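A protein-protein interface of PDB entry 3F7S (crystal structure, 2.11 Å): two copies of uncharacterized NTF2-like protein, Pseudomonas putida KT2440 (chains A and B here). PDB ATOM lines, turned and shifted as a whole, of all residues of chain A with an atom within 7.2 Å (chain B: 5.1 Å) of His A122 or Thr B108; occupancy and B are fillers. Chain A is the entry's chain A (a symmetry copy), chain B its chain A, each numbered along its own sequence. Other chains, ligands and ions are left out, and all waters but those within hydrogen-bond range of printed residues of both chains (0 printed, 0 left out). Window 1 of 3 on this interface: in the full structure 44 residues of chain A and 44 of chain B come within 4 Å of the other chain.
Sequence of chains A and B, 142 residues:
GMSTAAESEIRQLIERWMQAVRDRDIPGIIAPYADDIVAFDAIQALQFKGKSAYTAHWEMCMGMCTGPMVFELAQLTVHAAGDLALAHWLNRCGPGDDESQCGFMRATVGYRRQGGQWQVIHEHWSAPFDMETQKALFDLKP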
ATOM      1  N   TYR A  33      12.717  -7.368  27.193  1.00  0.00           N
ATOM      2  CA  TYR A  33      13.410  -6.480  26.251  1.00  0.00           C
ATOM      3  C   TYR A  33      13.489  -7.107  24.868  1.00  0.00           C
ATOM      4  O   TYR A  33      13.876  -8.271  24.758  1.00  0.00           O
ATOM      5  CB  TYR A  33      14.807  -6.182  26.764  1.00  0.00           C
ATOM      6  CG  TYR A  33      14.907  -5.227  27.951  1.00  0.00           C
ATOM      7  CD1 TYR A  33      13.802  -4.514  28.429  1.00  0.00           C
ATOM      8  CD2 TYR A  33      16.141  -4.965  28.532  1.00  0.00           C
ATOM      9  CE1 TYR A  33      13.938  -3.603  29.456  1.00  0.00           C
ATOM     10  CE2 TYR A  33      16.269  -4.073  29.582  1.00  0.00           C
ATOM     11  CZ  TYR A  33      15.163  -3.380  30.028  1.00  0.00           C
ATOM     12  OH  TYR A  33      15.293  -2.449  31.051  1.00  0.00           O
ATOM     13  N   ALA A  34      13.150  -6.352  23.818  1.00  0.00           N
ATOM     14  CA  ALA A  34      13.435  -6.797  22.442  1.00  0.00           C
ATOM     15  C   ALA A  34      14.951  -6.909  22.240  1.00  0.00           C
ATOM     16  O   ALA A  34      15.752  -6.223  22.889  1.00  0.00           O
ATOM     17  CB  ALA A  34      12.825  -5.857  21.397  1.00  0.00           C
ATOM     18  N   ASP A  36      16.623  -5.821  19.804  1.00  0.00           N
ATOM     19  CA  ASP A  36      17.124  -4.578  19.233  1.00  0.00           C
ATOM     20  C   ASP A  36      16.714  -3.327  20.037  1.00  0.00           C
ATOM     21  O   ASP A  36      16.711  -2.224  19.480  1.00  0.00           O
ATOM     22  CB  ASP A  36      16.711  -4.466  17.753  1.00  0.00           C
ATOM     23  CG  ASP A  36      15.189  -4.391  17.540  1.00  0.00           C
ATOM     24  OD1 ASP A  36      14.365  -4.751  18.430  1.00  0.00           O
ATOM     25  OD2 ASP A  36      14.801  -3.949  16.434  1.00  0.00           O
ATOM     26  N   ILE A  37      16.425  -3.497  21.339  1.00  0.00           N
ATOM     27  CA  ILE A  37      16.061  -2.382  22.227  1.00  0.00           C
ATOM     28  C   ILE A  37      17.072  -1.226  22.079  1.00  0.00           C
ATOM     29  O   ILE A  37      18.269  -1.459  21.977  1.00  0.00           O
ATOM     30  CB  ILE A  37      15.976  -2.866  23.677  1.00  0.00           C
ATOM     31  CG1 ILE A  37      15.503  -1.733  24.645  1.00  0.00           C
ATOM     32  CG2 ILE A  37      17.354  -3.488  24.083  1.00  0.00           C
ATOM     33  CD1 ILE A  37      15.001  -2.231  26.068  1.00  0.00           C
ATOM     34  N   VAL A  38      16.572   0.012  21.993  1.00  0.00           N
ATOM     35  CA  VAL A  38      17.420   1.221  22.066  1.00  0.00           C
ATOM     36  C   VAL A  38      17.077   1.983  23.322  1.00  0.00           C
ATOM     37  O   VAL A  38      15.899   2.386  23.513  1.00  0.00           O
ATOM     38  CB  VAL A  38      17.232   2.148  20.864  1.00  0.00           C
ATOM     39  CG1 VAL A  38      18.078   3.420  21.032  1.00  0.00           C
ATOM     40  CG2 VAL A  38      17.623   1.434  19.552  1.00  0.00           C
ATOM     41  N   ALA A  39      18.074   2.208  24.186  1.00  0.00           N
ATOM     42  CA  ALA A  39      17.813   2.822  25.522  1.00  0.00           C
ATOM     43  C   ALA A  39      18.655   4.058  25.718  1.00  0.00           C
ATOM     44  O   ALA A  39      19.850   4.019  25.465  1.00  0.00           O
ATOM     45  CB  ALA A  39      18.098   1.810  26.676  1.00  0.00           C
ATOM     46  N   PHE A  40      18.029   5.157  26.141  1.00  0.00           N
ATOM     47  CA  PHE A  40      18.717   6.345  26.613  1.00  0.00           C
ATOM     48  C   PHE A  40      18.651   6.333  28.131  1.00  0.00           C
ATOM     49  O   PHE A  40      17.582   6.625  28.721  1.00  0.00           O
ATOM     50  CB  PHE A  40      18.013   7.605  26.107  1.00  0.00           C
ATOM     51  CG  PHE A  40      17.840   7.680  24.598  1.00  0.00           C
ATOM     52  CD1 PHE A  40      18.739   7.068  23.721  1.00  0.00           C
ATOM     53  CD2 PHE A  40      16.789   8.420  24.065  1.00  0.00           C
ATOM     54  CE1 PHE A  40      18.577   7.173  22.359  1.00  0.00           C
ATOM     55  CE2 PHE A  40      16.644   8.576  22.713  1.00  0.00           C
ATOM     56  CZ  PHE A  40      17.540   7.927  21.840  1.00  0.00           C
ATOM     57  N   TYR A  54      22.849  -3.456  26.460  1.00  0.00           N
ATOM     58  CA  TYR A  54      22.049  -2.846  27.566  1.00  0.00           C
ATOM     59  C   TYR A  54      22.037  -3.769  28.784  1.00  0.00           C
ATOM     60  O   TYR A  54      22.052  -3.308  29.951  1.00  0.00           O
ATOM     61  CB  TYR A  54      20.607  -2.534  27.117  1.00  0.00           C
ATOM     62  CG  TYR A  54      19.829  -1.593  28.018  1.00  0.00           C
ATOM     63  CD1 TYR A  54      20.440  -0.465  28.617  1.00  0.00           C
ATOM     64  CD2 TYR A  54      18.468  -1.791  28.235  1.00  0.00           C
ATOM     65  CE1 TYR A  54      19.715   0.425  29.371  1.00  0.00           C
ATOM     66  CE2 TYR A  54      17.723  -0.876  29.015  1.00  0.00           C
ATOM     67  CZ  TYR A  54      18.345   0.201  29.583  1.00  0.00           C
ATOM     68  OH  TYR A  54      17.585   1.083  30.358  1.00  0.00           O
ATOM     69  N   LEU A  86       2.908   3.021  24.448  1.00  0.00           N
ATOM     70  CA  LEU A  86       3.738   4.043  25.033  1.00  0.00           C
ATOM     71  C   LEU A  86       3.382   4.177  26.533  1.00  0.00           C
ATOM     72  O   LEU A  86       2.204   4.237  26.875  1.00  0.00           O
ATOM     73  CB  LEU A  86       3.405   5.376  24.331  1.00  0.00           C
ATOM     74  CG  LEU A  86       4.020   6.592  25.014  1.00  0.00           C
ATOM     75  CD1 LEU A  86       5.530   6.615  24.613  1.00  0.00           C
ATOM     76  CD2 LEU A  86       3.280   7.863  24.661  1.00  0.00           C
ATOM     77  N   ALA A  87       4.371   4.299  27.399  1.00  0.00           N
ATOM     78  CA  ALA A  87       4.133   4.677  28.796  1.00  0.00           C
ATOM     79  C   ALA A  87       5.142   5.727  29.251  1.00  0.00           C
ATOM     80  O   ALA A  87       6.259   5.851  28.690  1.00  0.00           O
ATOM     81  CB  ALA A  87       4.182   3.450  29.687  1.00  0.00           C
ATOM     82  N   THR A 108      10.267   7.321  30.124  1.00  0.00           N
ATOM     83  CA  THR A 108       9.420   7.024  28.972  1.00  0.00           C
ATOM     84  C   THR A 108       9.778   5.661  28.396  1.00  0.00           C
ATOM     85  O   THR A 108      10.967   5.370  28.246  1.00  0.00           O
ATOM     86  CB  THR A 108       9.616   8.075  27.893  1.00  0.00           C
ATOM     87  OG1 THR A 108       9.363   9.372  28.469  1.00  0.00           O
ATOM     88  CG2 THR A 108       8.662   7.820  26.710  1.00  0.00           C
ATOM     89  N   VAL A 109       8.764   4.834  28.061  1.00  0.00           N
ATOM     90  CA  VAL A 109       9.027   3.490  27.521  1.00  0.00           C
ATOM     91  C   VAL A 109       8.104   3.234  26.352  1.00  0.00           C
ATOM     92  O   VAL A 109       6.896   3.550  26.404  1.00  0.00           O
ATOM     93  CB  VAL A 109       8.820   2.386  28.587  1.00  0.00           C
ATOM     94  CG1 VAL A 109       9.283   0.981  28.076  1.00  0.00           C
ATOM     95  CG2 VAL A 109       9.564   2.780  29.888  1.00  0.00           C
ATOM     96  N   GLY A 110       8.692   2.674  25.297  1.00  0.00           N
ATOM     97  CA  GLY A 110       7.958   2.247  24.110  1.00  0.00           C
ATOM     98  C   GLY A 110       7.946   0.738  23.965  1.00  0.00           C
ATOM     99  O   GLY A 110       8.959   0.037  24.238  1.00  0.00           O
ATOM    100  N   TYR A 111       6.788   0.224  23.548  1.00  0.00           N
ATOM    101  CA  TYR A 111       6.544  -1.217  23.511  1.00  0.00           C
ATOM    102  C   TYR A 111       5.999  -1.603  22.139  1.00  0.00           C
ATOM    103  O   TYR A 111       5.368  -0.785  21.454  1.00  0.00           O
ATOM    104  CB  TYR A 111       5.528  -1.662  24.583  1.00  0.00           C
ATOM    105  CG  TYR A 111       5.815  -1.210  26.013  1.00  0.00           C
ATOM    106  CD1 TYR A 111       5.439   0.047  26.432  1.00  0.00           C
ATOM    107  CD2 TYR A 111       6.431  -2.071  26.949  1.00  0.00           C
ATOM    108  CE1 TYR A 111       5.664   0.471  27.725  1.00  0.00           C
ATOM    109  CE2 TYR A 111       6.696  -1.639  28.248  1.00  0.00           C
ATOM    110  CZ  TYR A 111       6.324  -0.358  28.611  1.00  0.00           C
ATOM    111  OH  TYR A 111       6.546   0.132  29.873  1.00  0.00           O
ATOM    112  N   ARG A 112       6.262  -2.834  21.744  1.00  0.00           N
ATOM    113  CA  ARG A 112       5.768  -3.405  20.486  1.00  0.00           C
ATOM    114  C   ARG A 112       5.323  -4.846  20.647  1.00  0.00           C
ATOM    115  O   ARG A 112       6.022  -5.652  21.299  1.00  0.00           O
ATOM    116  CB  ARG A 112       6.874  -3.393  19.456  1.00  0.00           C
ATOM    117  CG  ARG A 112       6.439  -3.914  18.094  1.00  0.00           C
ATOM    118  CD  ARG A 112       7.448  -3.533  17.018  1.00  0.00           C
ATOM    119  NE  ARG A 112       6.995  -4.054  15.723  1.00  0.00           N
ATOM    120  CZ  ARG A 112       7.531  -3.756  14.537  1.00  0.00           C
ATOM    121  NH1 ARG A 112       8.562  -2.911  14.447  1.00  0.00           N
ATOM    122  NH2 ARG A 112       7.016  -4.301  13.434  1.00  0.00           N
ATOM    123  N   GLN A 119       6.950  -6.494  23.941  1.00  0.00           N
ATOM    124  CA  GLN A 119       8.335  -6.323  24.262  1.00  0.00           C
ATOM    125  C   GLN A 119       8.670  -4.850  24.340  1.00  0.00           C
ATOM    126  O   GLN A 119       8.057  -4.032  23.645  1.00  0.00           O
ATOM    127  CB  GLN A 119       9.182  -6.992  23.189  1.00  0.00           C
ATOM    128  CG  GLN A 119       9.022  -8.491  23.187  1.00  0.00           C
ATOM    129  CD  GLN A 119      10.144  -9.123  22.400  1.00  0.00           C
ATOM    130  OE1 GLN A 119      10.455  -8.681  21.294  1.00  0.00           O
ATOM    131  NE2 GLN A 119      10.810 -10.105  22.994  1.00  0.00           N
ATOM    132  N   VAL A 120       9.632  -4.514  25.201  1.00  0.00           N
ATOM    133  CA  VAL A 120      10.174  -3.145  25.291  1.00  0.00           C
ATOM    134  C   VAL A 120      11.150  -2.925  24.139  1.00  0.00           C
ATOM    135  O   VAL A 120      12.164  -3.646  24.012  1.00  0.00           O
ATOM    136  CB  VAL A 120      10.962  -2.893  26.586  1.00  0.00           C
ATOM    137  CG1 VAL A 120      11.476  -1.435  26.602  1.00  0.00           C
ATOM    138  CG2 VAL A 120      10.104  -3.224  27.838  1.00  0.00           C
ATOM    139  N   ILE A 121      10.844  -1.934  23.318  1.00  0.00           N
ATOM    140  CA  ILE A 121      11.702  -1.555  22.215  1.00  0.00           C
ATOM    141  C   ILE A 121      12.485  -0.257  22.484  1.00  0.00           C
ATOM    142  O   ILE A 121      13.472  -0.023  21.813  1.00  0.00           O
ATOM    143  CB  ILE A 121      10.941  -1.489  20.858  1.00  0.00           C
ATOM    144  CG1 ILE A 121       9.778  -0.497  20.895  1.00  0.00           C
ATOM    145  CG2 ILE A 121      10.574  -2.966  20.368  1.00  0.00           C
ATOM    146  CD1 ILE A 121       9.411   0.060  19.538  1.00  0.00           C
ATOM    147  N   HIS A 122      12.113   0.523  23.506  1.00  0.00           N
ATOM    148  CA  HIS A 122      12.781   1.789  23.794  1.00  0.00           C
ATOM    149  C   HIS A 122      12.538   2.200  25.234  1.00  0.00           C
ATOM    150  O   HIS A 122      11.441   1.993  25.733  1.00  0.00           O
ATOM    151  CB  HIS A 122      12.239   2.873  22.839  1.00  0.00           C
ATOM    152  CG  HIS A 122      12.819   4.244  23.052  1.00  0.00           C
ATOM    153  ND1 HIS A 122      14.164   4.518  22.935  1.00  0.00           N
ATOM    154  CD2 HIS A 122      12.220   5.429  23.349  1.00  0.00           C
ATOM    155  CE1 HIS A 122      14.367   5.816  23.152  1.00  0.00           C
ATOM    156  NE2 HIS A 122      13.200   6.389  23.413  1.00  0.00           N
ATOM    157  N   GLU A 123      13.575   2.758  25.881  1.00  0.00           N
ATOM    158  CA  GLU A 123      13.503   3.389  27.216  1.00  0.00           C
ATOM    159  C   GLU A 123      14.272   4.726  27.163  1.00  0.00           C
ATOM    160  O   GLU A 123      15.260   4.844  26.467  1.00  0.00           O
ATOM    161  CB  GLU A 123      14.171   2.522  28.295  1.00  0.00           C
ATOM    162  CG  GLU A 123      13.433   1.274  28.664  1.00  0.00           C
ATOM    163  CD  GLU A 123      14.072   0.488  29.793  1.00  0.00           C
ATOM    164  OE1 GLU A 123      15.103   0.950  30.331  1.00  0.00           O
ATOM    165  OE2 GLU A 123      13.547  -0.613  30.111  1.00  0.00           O
ATOM    166  N   HIS A 124      13.824   5.716  27.925  1.00  0.00           N
ATOM    167  CA  HIS A 124      14.490   7.035  28.066  1.00  0.00           C
ATOM    168  C   HIS A 124      14.284   7.389  29.526  1.00  0.00           C
ATOM    169  O   HIS A 124      13.146   7.569  29.972  1.00  0.00           O
ATOM    170  CB  HIS A 124      13.812   8.048  27.128  1.00  0.00           C
ATOM    171  CG  HIS A 124      14.517   9.366  26.960  1.00  0.00           C
ATOM    172  ND1 HIS A 124      15.434   9.867  27.862  1.00  0.00           N
ATOM    173  CD2 HIS A 124      14.372  10.322  26.006  1.00  0.00           C
ATOM    174  CE1 HIS A 124      15.869  11.046  27.435  1.00  0.00           C
ATOM    175  NE2 HIS A 124      15.232  11.352  26.321  1.00  0.00           N
ATOM    176  N   TRP A 125      15.394   7.461  30.256  1.00  0.00           N
ATOM    177  CA  TRP A 125      15.452   7.803  31.635  1.00  0.00           C
ATOM    178  C   TRP A 125      16.291   9.056  31.751  1.00  0.00           C
ATOM    179  O   TRP A 125      17.343   9.160  31.118  1.00  0.00           O
ATOM    180  CB  TRP A 125      16.171   6.667  32.405  1.00  0.00           C
ATOM    181  CG  TRP A 125      15.430   5.400  32.479  1.00  0.00           C
ATOM    182  CD1 TRP A 125      15.511   4.323  31.598  1.00  0.00           C
ATOM    183  CD2 TRP A 125      14.481   5.021  33.490  1.00  0.00           C
ATOM    184  NE1 TRP A 125      14.649   3.331  32.010  1.00  0.00           N
ATOM    185  CE2 TRP A 125      14.029   3.721  33.176  1.00  0.00           C
ATOM    186  CE3 TRP A 125      13.998   5.637  34.637  1.00  0.00           C
ATOM    187  CZ2 TRP A 125      13.100   3.044  33.977  1.00  0.00           C
ATOM    188  CZ3 TRP A 125      13.078   4.943  35.436  1.00  0.00           C
ATOM    189  CH2 TRP A 125      12.629   3.686  35.086  1.00  0.00           C
ATOM    190  N   LEU B  86       5.344   6.467  17.910  1.00  0.00           N
ATOM    191  CA  LEU B  86       6.495   6.725  18.738  1.00  0.00           C
ATOM    192  C   LEU B  86       7.682   7.128  17.831  1.00  0.00           C
ATOM    193  O   LEU B  86       7.930   6.467  16.826  1.00  0.00           O
ATOM    194  CB  LEU B  86       6.856   5.410  19.460  1.00  0.00           C
ATOM    195  CG  LEU B  86       8.202   5.459  20.175  1.00  0.00           C
ATOM    196  CD1 LEU B  86       7.978   6.267  21.494  1.00  0.00           C
ATOM    197  CD2 LEU B  86       8.764   4.074  20.402  1.00  0.00           C
ATOM    198  N   ALA B  87       8.444   8.136  18.213  1.00  0.00           N
ATOM    199  CA  ALA B  87       9.723   8.430  17.559  1.00  0.00           C
ATOM    200  C   ALA B  87      10.803   8.729  18.593  1.00  0.00           C
ATOM    201  O   ALA B  87      10.515   9.139  19.744  1.00  0.00           O
ATOM    202  CB  ALA B  87       9.562   9.584  16.587  1.00  0.00           C
ATOM    203  N   HIS B  88      12.047   8.454  18.213  1.00  0.00           N
ATOM    204  CA  HIS B  88      13.204   8.842  19.002  1.00  0.00           C
ATOM    205  C   HIS B  88      14.413   9.158  18.127  1.00  0.00           C
ATOM    206  O   HIS B  88      14.515   8.653  17.021  1.00  0.00           O
ATOM    207  CB  HIS B  88      13.541   7.824  20.106  1.00  0.00           C
ATOM    208  CG  HIS B  88      13.824   6.416  19.654  1.00  0.00           C
ATOM    209  ND1 HIS B  88      15.065   6.003  19.206  1.00  0.00           N
ATOM    210  CD2 HIS B  88      13.048   5.295  19.690  1.00  0.00           C
ATOM    211  CE1 HIS B  88      15.021   4.703  18.931  1.00  0.00           C
ATOM    212  NE2 HIS B  88      13.815   4.246  19.239  1.00  0.00           N
ATOM    213  N   ARG B 106      19.244  13.703  23.727  1.00  0.00           N
ATOM    214  CA  ARG B 106      18.328  12.650  23.319  1.00  0.00           C
ATOM    215  C   ARG B 106      16.873  13.146  23.320  1.00  0.00           C
ATOM    216  O   ARG B 106      16.485  13.940  24.200  1.00  0.00           O
ATOM    217  CB  ARG B 106      18.411  11.483  24.301  1.00  0.00           C
ATOM    218  CG  ARG B 106      19.773  10.849  24.471  1.00  0.00           C
ATOM    219  CD  ARG B 106      20.563  11.529  25.560  1.00  0.00           C
ATOM    220  NE  ARG B 106      19.972  11.461  26.882  1.00  0.00           N
ATOM    221  CZ  ARG B 106      20.125  10.483  27.760  1.00  0.00           C
ATOM    222  NH1 ARG B 106      20.834   9.414  27.468  1.00  0.00           N
ATOM    223  NH2 ARG B 106      19.548  10.580  28.952  1.00  0.00           N
ATOM    224  N   ALA B 107      16.085  12.610  22.375  1.00  0.00           N
ATOM    225  CA  ALA B 107      14.707  12.942  22.199  1.00  0.00           C
ATOM    226  C   ALA B 107      13.842  11.707  22.016  1.00  0.00           C
ATOM    227  O   ALA B 107      14.160  10.836  21.205  1.00  0.00           O
ATOM    228  CB  ALA B 107      14.544  13.864  20.966  1.00  0.00           C
ATOM    229  N   THR B 108      12.717  11.681  22.740  1.00  0.00           N
ATOM    230  CA  THR B 108      11.632  10.730  22.514  1.00  0.00           C
ATOM    231  C   THR B 108      10.305  11.467  22.399  1.00  0.00           C
ATOM    232  O   THR B 108      10.045  12.358  23.211  1.00  0.00           O
ATOM    233  CB  THR B 108      11.546   9.750  23.671  1.00  0.00           C
ATOM    234  OG1 THR B 108      12.833   9.120  23.832  1.00  0.00           O
ATOM    235  CG2 THR B 108      10.462   8.688  23.400  1.00  0.00           C
ATOM    236  N   VAL B 109       9.463  11.095  21.411  1.00  0.00           N
ATOM    237  CA  VAL B 109       8.171  11.775  21.217  1.00  0.00           C
ATOM    238  C   VAL B 109       7.098  10.743  20.963  1.00  0.00           C
ATOM    239  O   VAL B 109       7.302   9.778  20.195  1.00  0.00           O
ATOM    240  CB  VAL B 109       8.213  12.772  20.033  1.00  0.00           C
ATOM    241  CG1 VAL B 109       6.910  13.636  19.945  1.00  0.00           C
ATOM    242  CG2 VAL B 109       9.469  13.670  20.159  1.00  0.00           C
ATOM    243  N   GLY B 110       5.964  10.950  21.628  1.00  0.00           N
ATOM    244  CA  GLY B 110       4.770  10.132  21.440  1.00  0.00           C
ATOM    245  C   GLY B 110       3.650  10.910  20.778  1.00  0.00           C
ATOM    246  O   GLY B 110       3.422  12.117  21.064  1.00  0.00           O
ATOM    247  N   HIS B 122       3.327  13.607  23.978  1.00  0.00           N
ATOM    248  CA  HIS B 122       4.416  13.475  24.943  1.00  0.00           C
ATOM    249  C   HIS B 122       5.748  13.768  24.280  1.00  0.00           C
ATOM    250  O   HIS B 122       5.937  13.388  23.133  1.00  0.00           O
ATOM    251  CB  HIS B 122       4.414  12.040  25.510  1.00  0.00           C
ATOM    252  CG  HIS B 122       5.514  11.754  26.495  1.00  0.00           C
ATOM    253  ND1 HIS B 122       5.663  12.445  27.677  1.00  0.00           N
ATOM    254  CD2 HIS B 122       6.505  10.822  26.478  1.00  0.00           C
ATOM    255  CE1 HIS B 122       6.702  11.949  28.346  1.00  0.00           C
ATOM    256  NE2 HIS B 122       7.235  10.966  27.633  1.00  0.00           N
ATOM    257  N   GLU B 123       6.642  14.457  25.009  1.00  0.00           N
ATOM    258  CA  GLU B 123       8.052  14.689  24.628  1.00  0.00           C
ATOM    259  C   GLU B 123       8.938  14.422  25.862  1.00  0.00           C
ATOM    260  O   GLU B 123       8.540  14.684  26.978  1.00  0.00           O
ATOM    261  CB  GLU B 123       8.295  16.145  24.199  1.00  0.00           C
ATOM    262  CG  GLU B 123       7.702  16.533  22.882  1.00  0.00           C
ATOM    263  CD  GLU B 123       8.036  17.948  22.446  1.00  0.00           C
ATOM    264  OE1 GLU B 123       8.784  18.634  23.177  1.00  0.00           O
ATOM    265  OE2 GLU B 123       7.513  18.372  21.380  1.00  0.00           O
ATOM    266  N   HIS B 124      10.150  13.925  25.644  1.00  0.00           N
ATOM    267  CA  HIS B 124      11.165  13.691  26.702  1.00  0.00           C
ATOM    268  C   HIS B 124      12.476  14.051  26.030  1.00  0.00           C
ATOM    269  O   HIS B 124      12.883  13.399  25.063  1.00  0.00           O
ATOM    270  CB  HIS B 124      11.123  12.213  27.126  1.00  0.00           C
ATOM    271  CG  HIS B 124      11.910  11.858  28.359  1.00  0.00           C
ATOM    272  ND1 HIS B 124      12.950  12.621  28.851  1.00  0.00           N
ATOM    273  CD2 HIS B 124      11.839  10.763  29.159  1.00  0.00           C
ATOM    274  CE1 HIS B 124      13.441  12.041  29.940  1.00  0.00           C
ATOM    275  NE2 HIS B 124      12.797  10.907  30.140  1.00  0.00           N
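Of the printed residues of chain B, Leu A86 touches Leu B86 (3.98 Å).
Of the printed residues of chain B, His A122 touches His B88 (3.5 Å) and Thr B108 (2.8 Å).
Of the printed residues of chain B, Trp A125 touches Arg B106 (3.4 Å).
The nearest residue of chain B that does not touch His A122 is Leu B86 (4.4 Å).
The nearest printed residue of chain A that does not touch His B124 is Trp A125 (4.3 Å).
Leu A86 touches its own counterpart, Leu B86.
Thr A108 touches its own counterpart, Thr B108.
Thr A108 touches His B122, and with the chains exchanged His A122 touches Thr B108.
Thr A108 touches His B124, and with the chains exchanged His A124 touches Thr B108.
8 positions are printed for both chains.
Of the 13 pairs that touch across the chains among the printed residues, 7 have their exchanged pair printed and touching as well.
O of His A124 lies within hydrogen-bond range of N of Thr A108 (2.9 Å).
N of Val A38 is in hydrogen-bond range of O of Ile A121 (3.1 Å).
The backbone NH (N) of Trp A125 sits at hydrogen-bond distance from the backbone carbonyl oxygen (O) of Phe A40, 2.8 Å away.
The backbone NH (N) of Gly B110 sits at hydrogen-bond distance from the backbone carbonyl oxygen (O) of His B122, at 2.9 Å.
The backbone NH (N) of Glu A123 lies within hydrogen-bond range of the backbone carbonyl oxygen (O) of Val A38 (3.3 Å).
The backbone NH (N) of Thr B108 sits at hydrogen-bond distance from the backbone carbonyl oxygen (O) of His B124.
The backbone carbonyl oxygen (O) of Trp A125 is in hydrogen-bond range of the guanidinium group (NH2) of Arg B106, at 3.4 Å.
The backbone carbonyl oxygen (O) of His B124 sits at hydrogen-bond distance from a ring nitrogen (NE2) of His A124, 3.4 Å away.
A ring nitrogen (NE2) of His B122 lies within hydrogen-bond range of the side-chain hydroxyl (OG1) of Thr A108 (2.8 Å).
The side-chain hydroxyl of Thr B108 sits at hydrogen-bond distance from a ring nitrogen (NE2) of His A122 (2.8 Å).
Val A38 touches His B88 (CB to CE1, 3.9 Å).
CD2 of Phe A40 touches CB of Arg B106, 3.5 Å away.
Phe A40 touches Ala B107.
Leu A86 touches Leu B86.
Thr A108 touches Thr B108 (CG2 to CG2, 3.9 Å).
His B124 touches Thr A108 (CD2 to OG1, 2.9 Å).
ND1 of His A122 touches CD2 of His B88, 3.5 Å away.
O of Arg B106 touches NE2 of His A124 (3.6 Å).
Thr B108 touches His A124 (OG1 to CD2, 2.9 Å).
Along chain B the printed residues that touch a printed residue of chain A span positions 86 to 124.
Hydrophobic or aromatic side chains of chain A within 4 Å of the printed part of chain B: Val A38, Phe A40, Leu A86, His A122 and His A124.
Among the printed residues, 13 pairs touch across the chains.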
